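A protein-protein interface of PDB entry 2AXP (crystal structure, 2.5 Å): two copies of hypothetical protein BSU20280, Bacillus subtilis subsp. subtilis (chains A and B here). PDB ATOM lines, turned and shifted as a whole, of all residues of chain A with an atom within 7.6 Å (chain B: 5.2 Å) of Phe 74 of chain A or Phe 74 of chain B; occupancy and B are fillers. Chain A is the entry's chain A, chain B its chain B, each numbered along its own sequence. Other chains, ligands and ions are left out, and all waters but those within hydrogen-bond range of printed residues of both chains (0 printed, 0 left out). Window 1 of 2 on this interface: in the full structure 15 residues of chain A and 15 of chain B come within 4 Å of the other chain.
The side-chain amino group (NZ) of Lys 73 of chain A is in salt-bridge range of the side-chain carboxylate (OD1) of Asp 124 of chain A, at 3.6 Å.
The backbone carbonyl oxygen of Ala 71 of chain A lies within hydrogen-bond range of the side-chain amino group of Lys 75 of chain B, 3.0 Å away.
O of Lys 73 of chain A is in hydrogen-bond range of N of Lys 75 of chain B (3.0 Å).
The side-chain amino group (NZ) of Lys 75 of chain A sits at hydrogen-bond distance from the backbone carbonyl oxygen (O) of Ala 71 of chain B (2.9 Å).
The backbone carbonyl oxygen of Lys 73 of chain B sits at hydrogen-bond distance from the backbone NH of Lys 75 of chain A (3.0 Å).
Of the 18 printed residues of chain A, 6 touch a printed residue of chain B.
Hydrophobic or aromatic side chains of chain A that line the printed part of chain B: Phe 74.
Along chain A the printed residues that touch a printed residue of chain B span positions 71 to 124.
Hydrophobic or aromatic side chains of chain B that line the printed part of chain A: Phe 35 and Phe 74.
Ala 71 of chain A touches Lys 75 of chain B, and with the chains exchanged Lys 75 of chain A touches Ala 71 of chain B.
Lys 73 of chain A touches Phe 74 of chain B, and with the chains exchanged Phe 74 of chain A touches Lys 73 of chain B.
Phe 74 of chain B touches its own counterpart, Phe 74 of chain A.
Phe 74 of chain A touches Lys 75 of chain B, and with the chains exchanged Lys 75 of chain A touches Phe 74 of chain B.
9 positions are printed for both chains.
Printed residues of chain B within 4 Å of Phe 74 of chain A: Lys 73, Phe 74 and Lys 75.
Of chain A, only Lys 73, Phe 74 and Lys 75 come within 4 Å of Phe 74 of chain B.
Of the printed residues of chain B, Lys 73 of chain A touches Phe 74 and Lys 75.
Of the printed residues of chain B, Lys 75 of chain A touches Ala 71, Lys 73, Phe 74 and Lys 75.
The nearest printed residue of chain B that does not touch Phe 74 of chain A is Lys 72 of chain B (7.4 Å).
CA of Phe 74 of chain B touches O of Lys 73 of chain A (3.4 Å).
Lys 73 of chain B touches Phe 74 of chain A.
Phe 74 of chain A touches Phe 74 of chain B (CE1 to CE1, 3.8 Å).
Lys 75 of chain B touches Phe 74 of chain A (CE to O, 3.2 Å).
CE of Lys 75 of chain A touches O of Phe 74 of chain B, 3.1 Å away.
Lys 75 of chain B touches Lys 75 of chain A.
Glu 121 of chain A touches Phe 35 of chain B (CG to CD2, 3.4 Å).
OD1 of Asp 124 of chain A touches CE2 of Phe 35 of chain B (3.7 Å).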
ATOM      1  N   PHE A  35       4.877 -17.314  21.278  1.00  0.00           N
ATOM      2  CA  PHE A  35       3.430 -17.515  21.245  1.00  0.00           C
ATOM      3  C   PHE A  35       3.015 -18.520  22.307  1.00  0.00           C
ATOM      4  O   PHE A  35       2.082 -18.279  23.076  1.00  0.00           O
ATOM      5  CB  PHE A  35       2.975 -18.010  19.868  1.00  0.00           C
ATOM      6  CG  PHE A  35       1.480 -18.182  19.747  1.00  0.00           C
ATOM      7  CD1 PHE A  35       0.630 -17.076  19.787  1.00  0.00           C
ATOM      8  CD2 PHE A  35       0.920 -19.454  19.618  1.00  0.00           C
ATOM      9  CE1 PHE A  35      -0.757 -17.235  19.702  1.00  0.00           C
ATOM     10  CE2 PHE A  35      -0.466 -19.624  19.532  1.00  0.00           C
ATOM     11  CZ  PHE A  35      -1.306 -18.513  19.574  1.00  0.00           C
ATOM     12  N   ALA A  38       3.594 -17.003  25.702  1.00  0.00           N
ATOM     13  CA  ALA A  38       2.776 -15.802  25.888  1.00  0.00           C
ATOM     14  C   ALA A  38       1.341 -16.192  26.227  1.00  0.00           C
ATOM     15  O   ALA A  38       0.518 -15.348  26.584  1.00  0.00           O
ATOM     16  CB  ALA A  38       2.801 -14.947  24.633  1.00  0.00           C
ATOM     17  N   LYS A  39       1.053 -17.484  26.100  1.00  0.00           N
ATOM     18  CA  LYS A  39      -0.267 -18.014  26.404  1.00  0.00           C
ATOM     19  C   LYS A  39      -0.253 -18.601  27.806  1.00  0.00           C
ATOM     20  O   LYS A  39      -1.080 -18.237  28.645  1.00  0.00           O
ATOM     21  CB  LYS A  39      -0.656 -19.093  25.388  1.00  0.00           C
ATOM     22  CG  LYS A  39      -1.162 -18.553  24.042  1.00  0.00           C
ATOM     23  CD  LYS A  39      -1.381 -19.687  23.028  1.00  0.00           C
ATOM     24  CE  LYS A  39      -2.348 -20.758  23.556  1.00  0.00           C
ATOM     25  NZ  LYS A  39      -2.398 -21.995  22.708  1.00  0.00           N
ATOM     26  N   VAL A  69       2.551  -5.415  22.171  1.00  0.00           N
ATOM     27  CA  VAL A  69       1.758  -5.002  21.019  1.00  0.00           C
ATOM     28  C   VAL A  69       0.835  -6.134  20.599  1.00  0.00           C
ATOM     29  O   VAL A  69      -0.376  -5.986  20.608  1.00  0.00           O
ATOM     30  CB  VAL A  69       2.675  -4.614  19.830  1.00  0.00           C
ATOM     31  CG1 VAL A  69       1.920  -4.707  18.518  1.00  0.00           C
ATOM     32  CG2 VAL A  69       3.187  -3.207  20.015  1.00  0.00           C
ATOM     33  N   TYR A  70       1.410  -7.270  20.237  1.00  0.00           N
ATOM     34  CA  TYR A  70       0.601  -8.387  19.822  1.00  0.00           C
ATOM     35  C   TYR A  70      -0.304  -8.907  20.933  1.00  0.00           C
ATOM     36  O   TYR A  70      -1.198  -9.713  20.682  1.00  0.00           O
ATOM     37  CB  TYR A  70       1.491  -9.509  19.290  1.00  0.00           C
ATOM     38  CG  TYR A  70       2.215  -9.132  18.018  1.00  0.00           C
ATOM     39  CD1 TYR A  70       1.504  -8.735  16.875  1.00  0.00           C
ATOM     40  CD2 TYR A  70       3.614  -9.125  17.963  1.00  0.00           C
ATOM     41  CE1 TYR A  70       2.170  -8.334  15.709  1.00  0.00           C
ATOM     42  CE2 TYR A  70       4.290  -8.727  16.807  1.00  0.00           C
ATOM     43  CZ  TYR A  70       3.563  -8.329  15.686  1.00  0.00           C
ATOM     44  OH  TYR A  70       4.227  -7.907  14.557  1.00  0.00           O
ATOM     45  N   ALA A  71      -0.086  -8.452  22.162  1.00  0.00           N
ATOM     46  CA  ALA A  71      -0.912  -8.909  23.284  1.00  0.00           C
ATOM     47  C   ALA A  71      -2.305  -8.289  23.216  1.00  0.00           C
ATOM     48  O   ALA A  71      -3.287  -8.905  23.628  1.00  0.00           O
ATOM     49  CB  ALA A  71      -0.249  -8.555  24.608  1.00  0.00           C
ATOM     50  N   LYS A  72      -2.372  -7.068  22.695  1.00  0.00           N
ATOM     51  CA  LYS A  72      -3.625  -6.343  22.560  1.00  0.00           C
ATOM     52  C   LYS A  72      -4.339  -6.809  21.304  1.00  0.00           C
ATOM     53  O   LYS A  72      -5.104  -6.055  20.714  1.00  0.00           O
ATOM     54  CB  LYS A  72      -3.364  -4.835  22.441  1.00  0.00           C
ATOM     55  CG  LYS A  72      -2.421  -4.247  23.490  1.00  0.00           C
ATOM     56  CD  LYS A  72      -2.978  -4.361  24.898  1.00  0.00           C
ATOM     57  CE  LYS A  72      -2.093  -3.632  25.897  1.00  0.00           C
ATOM     58  NZ  LYS A  72      -2.693  -3.619  27.265  1.00  0.00           N
ATOM     59  N   LYS A  73      -4.087  -8.041  20.879  1.00  0.00           N
ATOM     60  CA  LYS A  73      -4.729  -8.535  19.666  1.00  0.00           C
ATOM     61  C   LYS A  73      -5.183  -9.979  19.754  1.00  0.00           C
ATOM     62  O   LYS A  73      -6.213 -10.339  19.194  1.00  0.00           O
ATOM     63  CB  LYS A  73      -3.789  -8.367  18.465  1.00  0.00           C
ATOM     64  CG  LYS A  73      -3.571  -6.919  18.049  1.00  0.00           C
ATOM     65  CD  LYS A  73      -4.896  -6.262  17.662  1.00  0.00           C
ATOM     66  CE  LYS A  73      -4.735  -4.782  17.346  1.00  0.00           C
ATOM     67  NZ  LYS A  73      -6.041  -4.158  16.983  1.00  0.00           N
ATOM     68  N   PHE A  74      -4.419 -10.803  20.458  1.00  0.00           N
ATOM     69  CA  PHE A  74      -4.762 -12.208  20.590  1.00  0.00           C
ATOM     70  C   PHE A  74      -5.319 -12.545  21.969  1.00  0.00           C
ATOM     71  O   PHE A  74      -4.811 -12.067  22.985  1.00  0.00           O
ATOM     72  CB  PHE A  74      -3.531 -13.074  20.325  1.00  0.00           C
ATOM     73  CG  PHE A  74      -2.855 -12.792  19.017  1.00  0.00           C
ATOM     74  CD1 PHE A  74      -3.556 -12.892  17.820  1.00  0.00           C
ATOM     75  CD2 PHE A  74      -1.517 -12.425  18.983  1.00  0.00           C
ATOM     76  CE1 PHE A  74      -2.934 -12.633  16.606  1.00  0.00           C
ATOM     77  CE2 PHE A  74      -0.886 -12.164  17.776  1.00  0.00           C
ATOM     78  CZ  PHE A  74      -1.597 -12.266  16.586  1.00  0.00           C
ATOM     79  N   LYS A  75      -6.358 -13.375  21.995  1.00  0.00           N
ATOM     80  CA  LYS A  75      -6.971 -13.798  23.248  1.00  0.00           C
ATOM     81  C   LYS A  75      -6.010 -14.723  23.992  1.00  0.00           C
ATOM     82  O   LYS A  75      -5.188 -15.408  23.374  1.00  0.00           O
ATOM     83  CB  LYS A  75      -8.286 -14.536  22.978  1.00  0.00           C
ATOM     84  CG  LYS A  75      -9.424 -13.655  22.508  1.00  0.00           C
ATOM     85  CD  LYS A  75     -10.727 -14.449  22.380  1.00  0.00           C
ATOM     86  CE  LYS A  75     -11.915 -13.531  22.075  1.00  0.00           C
ATOM     87  NZ  LYS A  75     -13.184 -14.281  21.903  1.00  0.00           N
ATOM     88  N   ASP A  76      -6.114 -14.740  25.319  1.00  0.00           N
ATOM     89  CA  ASP A  76      -5.253 -15.586  26.140  1.00  0.00           C
ATOM     90  C   ASP A  76      -3.793 -15.315  25.777  1.00  0.00           C
ATOM     91  O   ASP A  76      -3.044 -16.221  25.393  1.00  0.00           O
ATOM     92  CB  ASP A  76      -5.586 -17.067  25.907  1.00  0.00           C
ATOM     93  CG  ASP A  76      -7.028 -17.415  26.276  1.00  0.00           C
ATOM     94  OD1 ASP A  76      -7.400 -18.605  26.176  1.00  0.00           O
ATOM     95  OD2 ASP A  76      -7.790 -16.500  26.663  1.00  0.00           O
ATOM     96  N   TYR A  77      -3.399 -14.050  25.901  1.00  0.00           N
ATOM     97  CA  TYR A  77      -2.043 -13.624  25.579  1.00  0.00           C
ATOM     98  C   TYR A  77      -1.545 -12.704  26.697  1.00  0.00           C
ATOM     99  O   TYR A  77      -2.088 -11.616  26.912  1.00  0.00           O
ATOM    100  CB  TYR A  77      -2.067 -12.897  24.229  1.00  0.00           C
ATOM    101  CG  TYR A  77      -0.764 -12.914  23.462  1.00  0.00           C
ATOM    102  CD1 TYR A  77       0.203 -11.932  23.674  1.00  0.00           C
ATOM    103  CD2 TYR A  77      -0.499 -13.916  22.528  1.00  0.00           C
ATOM    104  CE1 TYR A  77       1.404 -11.945  22.975  1.00  0.00           C
ATOM    105  CE2 TYR A  77       0.701 -13.942  21.820  1.00  0.00           C
ATOM    106  CZ  TYR A  77       1.650 -12.952  22.047  1.00  0.00           C
ATOM    107  OH  TYR A  77       2.844 -12.967  21.357  1.00  0.00           O
ATOM    108  N   SER A  78      -0.514 -13.149  27.413  1.00  0.00           N
ATOM    109  CA  SER A  78       0.035 -12.366  28.519  1.00  0.00           C
ATOM    110  C   SER A  78       0.814 -11.154  28.051  1.00  0.00           C
ATOM    111  O   SER A  78       1.289 -11.103  26.921  1.00  0.00           O
ATOM    112  CB  SER A  78       0.943 -13.229  29.396  1.00  0.00           C
ATOM    113  OG  SER A  78       0.216 -14.274  30.019  1.00  0.00           O
ATOM    114  N   ILE A  79       0.943 -10.181  28.940  1.00  0.00           N
ATOM    115  CA  ILE A  79       1.665  -8.950  28.653  1.00  0.00           C
ATOM    116  C   ILE A  79       2.562  -8.648  29.854  1.00  0.00           C
ATOM    117  O   ILE A  79       2.267  -9.068  30.981  1.00  0.00           O
ATOM    118  CB  ILE A  79       0.696  -7.765  28.484  1.00  0.00           C
ATOM    119  CG1 ILE A  79      -0.666  -8.286  28.032  1.00  0.00           C
ATOM    120  CG2 ILE A  79       1.253  -6.776  27.481  1.00  0.00           C
ATOM    121  CD1 ILE A  79      -1.770  -7.219  27.973  1.00  0.00           C
ATOM    122  N   TYR A 119      -6.243 -13.356   4.789  1.00  0.00           N
ATOM    123  CA  TYR A 119      -6.853 -12.830   6.016  1.00  0.00           C
ATOM    124  C   TYR A 119      -6.556 -11.333   6.135  1.00  0.00           C
ATOM    125  O   TYR A 119      -7.062 -10.658   7.033  1.00  0.00           O
ATOM    126  CB  TYR A 119      -6.281 -13.558   7.247  1.00  0.00           C
ATOM    127  CG  TYR A 119      -4.825 -13.222   7.546  1.00  0.00           C
ATOM    128  CD1 TYR A 119      -3.792 -13.663   6.703  1.00  0.00           C
ATOM    129  CD2 TYR A 119      -4.485 -12.426   8.647  1.00  0.00           C
ATOM    130  CE1 TYR A 119      -2.452 -13.312   6.949  1.00  0.00           C
ATOM    131  CE2 TYR A 119      -3.153 -12.068   8.902  1.00  0.00           C
ATOM    132  CZ  TYR A 119      -2.142 -12.512   8.049  1.00  0.00           C
ATOM    133  OH  TYR A 119      -0.837 -12.141   8.292  1.00  0.00           O
ATOM    134  N   GLU A 121      -6.549  -8.051   6.756  1.00  0.00           N
ATOM    135  CA  GLU A 121      -7.641  -7.178   7.172  1.00  0.00           C
ATOM    136  C   GLU A 121      -7.816  -6.023   6.183  1.00  0.00           C
ATOM    137  O   GLU A 121      -8.726  -6.044   5.342  1.00  0.00           O
ATOM    138  CB  GLU A 121      -7.385  -6.619   8.576  1.00  0.00           C
ATOM    139  CG  GLU A 121      -7.550  -7.626   9.713  1.00  0.00           C
ATOM    140  CD  GLU A 121      -6.459  -8.687   9.754  1.00  0.00           C
ATOM    141  OE1 GLU A 121      -5.260  -8.324   9.724  1.00  0.00           O
ATOM    142  OE2 GLU A 121      -6.799  -9.887   9.839  1.00  0.00           O
ATOM    143  N   ASP A 124      -6.285  -3.162  10.007  1.00  0.00           N
ATOM    144  CA  ASP A 124      -5.695  -3.665  11.239  1.00  0.00           C
ATOM    145  C   ASP A 124      -4.209  -3.315  11.272  1.00  0.00           C
ATOM    146  O   ASP A 124      -3.614  -3.152  12.339  1.00  0.00           O
ATOM    147  CB  ASP A 124      -5.849  -5.174  11.334  1.00  0.00           C
ATOM    148  CG  ASP A 124      -5.153  -5.737  12.541  1.00  0.00           C
ATOM    149  OD1 ASP A 124      -5.652  -5.509  13.669  1.00  0.00           O
ATOM    150  OD2 ASP A 124      -4.098  -6.385  12.355  1.00  0.00           O
ATOM    151  N   ILE A 128      -1.849  -1.773  14.151  1.00  0.00           N
ATOM    152  CA  ILE A 128      -0.587  -2.372  14.555  1.00  0.00           C
ATOM    153  C   ILE A 128       0.496  -1.308  14.520  1.00  0.00           C
ATOM    154  O   ILE A 128       1.246  -1.152  15.479  1.00  0.00           O
ATOM    155  CB  ILE A 128      -0.190  -3.557  13.629  1.00  0.00           C
ATOM    156  CG1 ILE A 128      -1.047  -4.784  13.968  1.00  0.00           C
ATOM    157  CG2 ILE A 128       1.295  -3.877  13.778  1.00  0.00           C
ATOM    158  CD1 ILE A 128      -0.685  -6.047  13.198  1.00  0.00           C
ATOM    159  N   PHE B  35     -13.583  -8.578   9.533  1.00  0.00           N
ATOM    160  CA  PHE B  35     -12.799  -8.265  10.728  1.00  0.00           C
ATOM    161  C   PHE B  35     -13.338  -6.996  11.372  1.00  0.00           C
ATOM    162  O   PHE B  35     -13.484  -6.917  12.595  1.00  0.00           O
ATOM    163  CB  PHE B  35     -11.317  -8.071  10.378  1.00  0.00           C
ATOM    164  CG  PHE B  35     -10.433  -7.827  11.581  1.00  0.00           C
ATOM    165  CD1 PHE B  35     -10.094  -8.872  12.440  1.00  0.00           C
ATOM    166  CD2 PHE B  35      -9.968  -6.542  11.873  1.00  0.00           C
ATOM    167  CE1 PHE B  35      -9.308  -8.641  13.575  1.00  0.00           C
ATOM    168  CE2 PHE B  35      -9.180  -6.298  13.007  1.00  0.00           C
ATOM    169  CZ  PHE B  35      -8.850  -7.350  13.860  1.00  0.00           C
ATOM    170  N   TYR B  70     -12.196 -17.978  13.907  1.00  0.00           N
ATOM    171  CA  TYR B  70     -11.300 -16.881  14.176  1.00  0.00           C
ATOM    172  C   TYR B  70     -11.729 -16.055  15.376  1.00  0.00           C
ATOM    173  O   TYR B  70     -10.965 -15.226  15.860  1.00  0.00           O
ATOM    174  CB  TYR B  70     -11.171 -15.997  12.935  1.00  0.00           C
ATOM    175  CG  TYR B  70     -10.499 -16.703  11.778  1.00  0.00           C
ATOM    176  CD1 TYR B  70      -9.210 -17.234  11.912  1.00  0.00           C
ATOM    177  CD2 TYR B  70     -11.162 -16.874  10.561  1.00  0.00           C
ATOM    178  CE1 TYR B  70      -8.599 -17.926  10.860  1.00  0.00           C
ATOM    179  CE2 TYR B  70     -10.564 -17.562   9.504  1.00  0.00           C
ATOM    180  CZ  TYR B  70      -9.285 -18.088   9.662  1.00  0.00           C
ATOM    181  OH  TYR B  70      -8.708 -18.795   8.635  1.00  0.00           O
ATOM    182  N   ALA B  71     -12.941 -16.277  15.874  1.00  0.00           N
ATOM    183  CA  ALA B  71     -13.422 -15.514  17.030  1.00  0.00           C
ATOM    184  C   ALA B  71     -12.728 -15.971  18.310  1.00  0.00           C
ATOM    185  O   ALA B  71     -12.515 -15.181  19.227  1.00  0.00           O
ATOM    186  CB  ALA B  71     -14.927 -15.664  17.173  1.00  0.00           C
ATOM    187  N   LYS B  72     -12.381 -17.254  18.354  1.00  0.00           N
ATOM    188  CA  LYS B  72     -11.712 -17.841  19.505  1.00  0.00           C
ATOM    189  C   LYS B  72     -10.224 -17.555  19.418  1.00  0.00           C
ATOM    190  O   LYS B  72      -9.417 -18.316  19.942  1.00  0.00           O
ATOM    191  CB  LYS B  72     -11.916 -19.363  19.523  1.00  0.00           C
ATOM    192  CG  LYS B  72     -13.360 -19.838  19.342  1.00  0.00           C
ATOM    193  CD  LYS B  72     -14.261 -19.389  20.482  1.00  0.00           C
ATOM    194  CE  LYS B  72     -15.648 -19.999  20.355  1.00  0.00           C
ATOM    195  NZ  LYS B  72     -16.510 -19.669  21.528  1.00  0.00           N
ATOM    196  N   LYS B  73      -9.848 -16.471  18.749  1.00  0.00           N
ATOM    197  CA  LYS B  73      -8.430 -16.155  18.612  1.00  0.00           C
ATOM    198  C   LYS B  73      -8.111 -14.680  18.754  1.00  0.00           C
ATOM    199  O   LYS B  73      -7.065 -14.320  19.290  1.00  0.00           O
ATOM    200  CB  LYS B  73      -7.904 -16.665  17.265  1.00  0.00           C
ATOM    201  CG  LYS B  73      -7.831 -18.184  17.167  1.00  0.00           C
ATOM    202  CD  LYS B  73      -6.902 -18.752  18.240  1.00  0.00           C
ATOM    203  CE  LYS B  73      -6.890 -20.273  18.244  1.00  0.00           C
ATOM    204  NZ  LYS B  73      -5.986 -20.804  19.304  1.00  0.00           N
ATOM    205  N   PHE B  74      -9.008 -13.827  18.281  1.00  0.00           N
ATOM    206  CA  PHE B  74      -8.787 -12.393  18.357  1.00  0.00           C
ATOM    207  C   PHE B  74      -9.640 -11.724  19.427  1.00  0.00           C
ATOM    208  O   PHE B  74     -10.822 -12.034  19.573  1.00  0.00           O
ATOM    209  CB  PHE B  74      -9.093 -11.746  17.006  1.00  0.00           C
ATOM    210  CG  PHE B  74      -8.353 -12.361  15.856  1.00  0.00           C
ATOM    211  CD1 PHE B  74      -6.961 -12.424  15.856  1.00  0.00           C
ATOM    212  CD2 PHE B  74      -9.047 -12.875  14.768  1.00  0.00           C
ATOM    213  CE1 PHE B  74      -6.272 -12.993  14.791  1.00  0.00           C
ATOM    214  CE2 PHE B  74      -8.368 -13.444  13.700  1.00  0.00           C
ATOM    215  CZ  PHE B  74      -6.976 -13.503  13.710  1.00  0.00           C
ATOM    216  N   LYS B  75      -9.034 -10.798  20.164  1.00  0.00           N
ATOM    217  CA  LYS B  75      -9.739 -10.069  21.207  1.00  0.00           C
ATOM    218  C   LYS B  75     -10.760  -9.133  20.565  1.00  0.00           C
ATOM    219  O   LYS B  75     -10.574  -8.689  19.428  1.00  0.00           O
ATOM    220  CB  LYS B  75      -8.755  -9.253  22.052  1.00  0.00           C
ATOM    221  CG  LYS B  75      -7.866 -10.073  22.966  1.00  0.00           C
ATOM    222  CD  LYS B  75      -7.018  -9.172  23.868  1.00  0.00           C
ATOM    223  CE  LYS B  75      -6.253  -9.989  24.912  1.00  0.00           C
ATOM    224  NZ  LYS B  75      -5.381  -9.140  25.766  1.00  0.00           N
ATOM    225  N   ASP B  76     -11.833  -8.836  21.297  1.00  0.00           N
ATOM    226  CA  ASP B  76     -12.878  -7.950  20.790  1.00  0.00           C
ATOM    227  C   ASP B  76     -13.350  -8.454  19.423  1.00  0.00           C
ATOM    228  O   ASP B  76     -13.308  -7.735  18.421  1.00  0.00           O
ATOM    229  CB  ASP B  76     -12.342  -6.515  20.668  1.00  0.00           C
ATOM    230  CG  ASP B  76     -11.884  -5.941  22.002  1.00  0.00           C
ATOM    231  OD1 ASP B  76     -11.487  -4.753  22.034  1.00  0.00           O
ATOM    232  OD2 ASP B  76     -11.919  -6.675  23.016  1.00  0.00           O
ATOM    233  N   TYR B  77     -13.795  -9.705  19.398  1.00  0.00           N
ATOM    234  CA  TYR B  77     -14.264 -10.333  18.169  1.00  0.00           C
ATOM    235  C   TYR B  77     -15.577 -11.068  18.465  1.00  0.00           C
ATOM    236  O   TYR B  77     -15.606 -12.026  19.247  1.00  0.00           O
ATOM    237  CB  TYR B  77     -13.183 -11.302  17.676  1.00  0.00           C
ATOM    238  CG  TYR B  77     -13.199 -11.587  16.196  1.00  0.00           C
ATOM    239  CD1 TYR B  77     -13.985 -12.612  15.672  1.00  0.00           C
ATOM    240  CD2 TYR B  77     -12.421 -10.831  15.316  1.00  0.00           C
ATOM    241  CE1 TYR B  77     -13.997 -12.881  14.307  1.00  0.00           C
ATOM    242  CE2 TYR B  77     -12.424 -11.087  13.948  1.00  0.00           C
ATOM    243  CZ  TYR B  77     -13.214 -12.116  13.448  1.00  0.00           C
ATOM    244  OH  TYR B  77     -13.229 -12.385  12.096  1.00  0.00           O
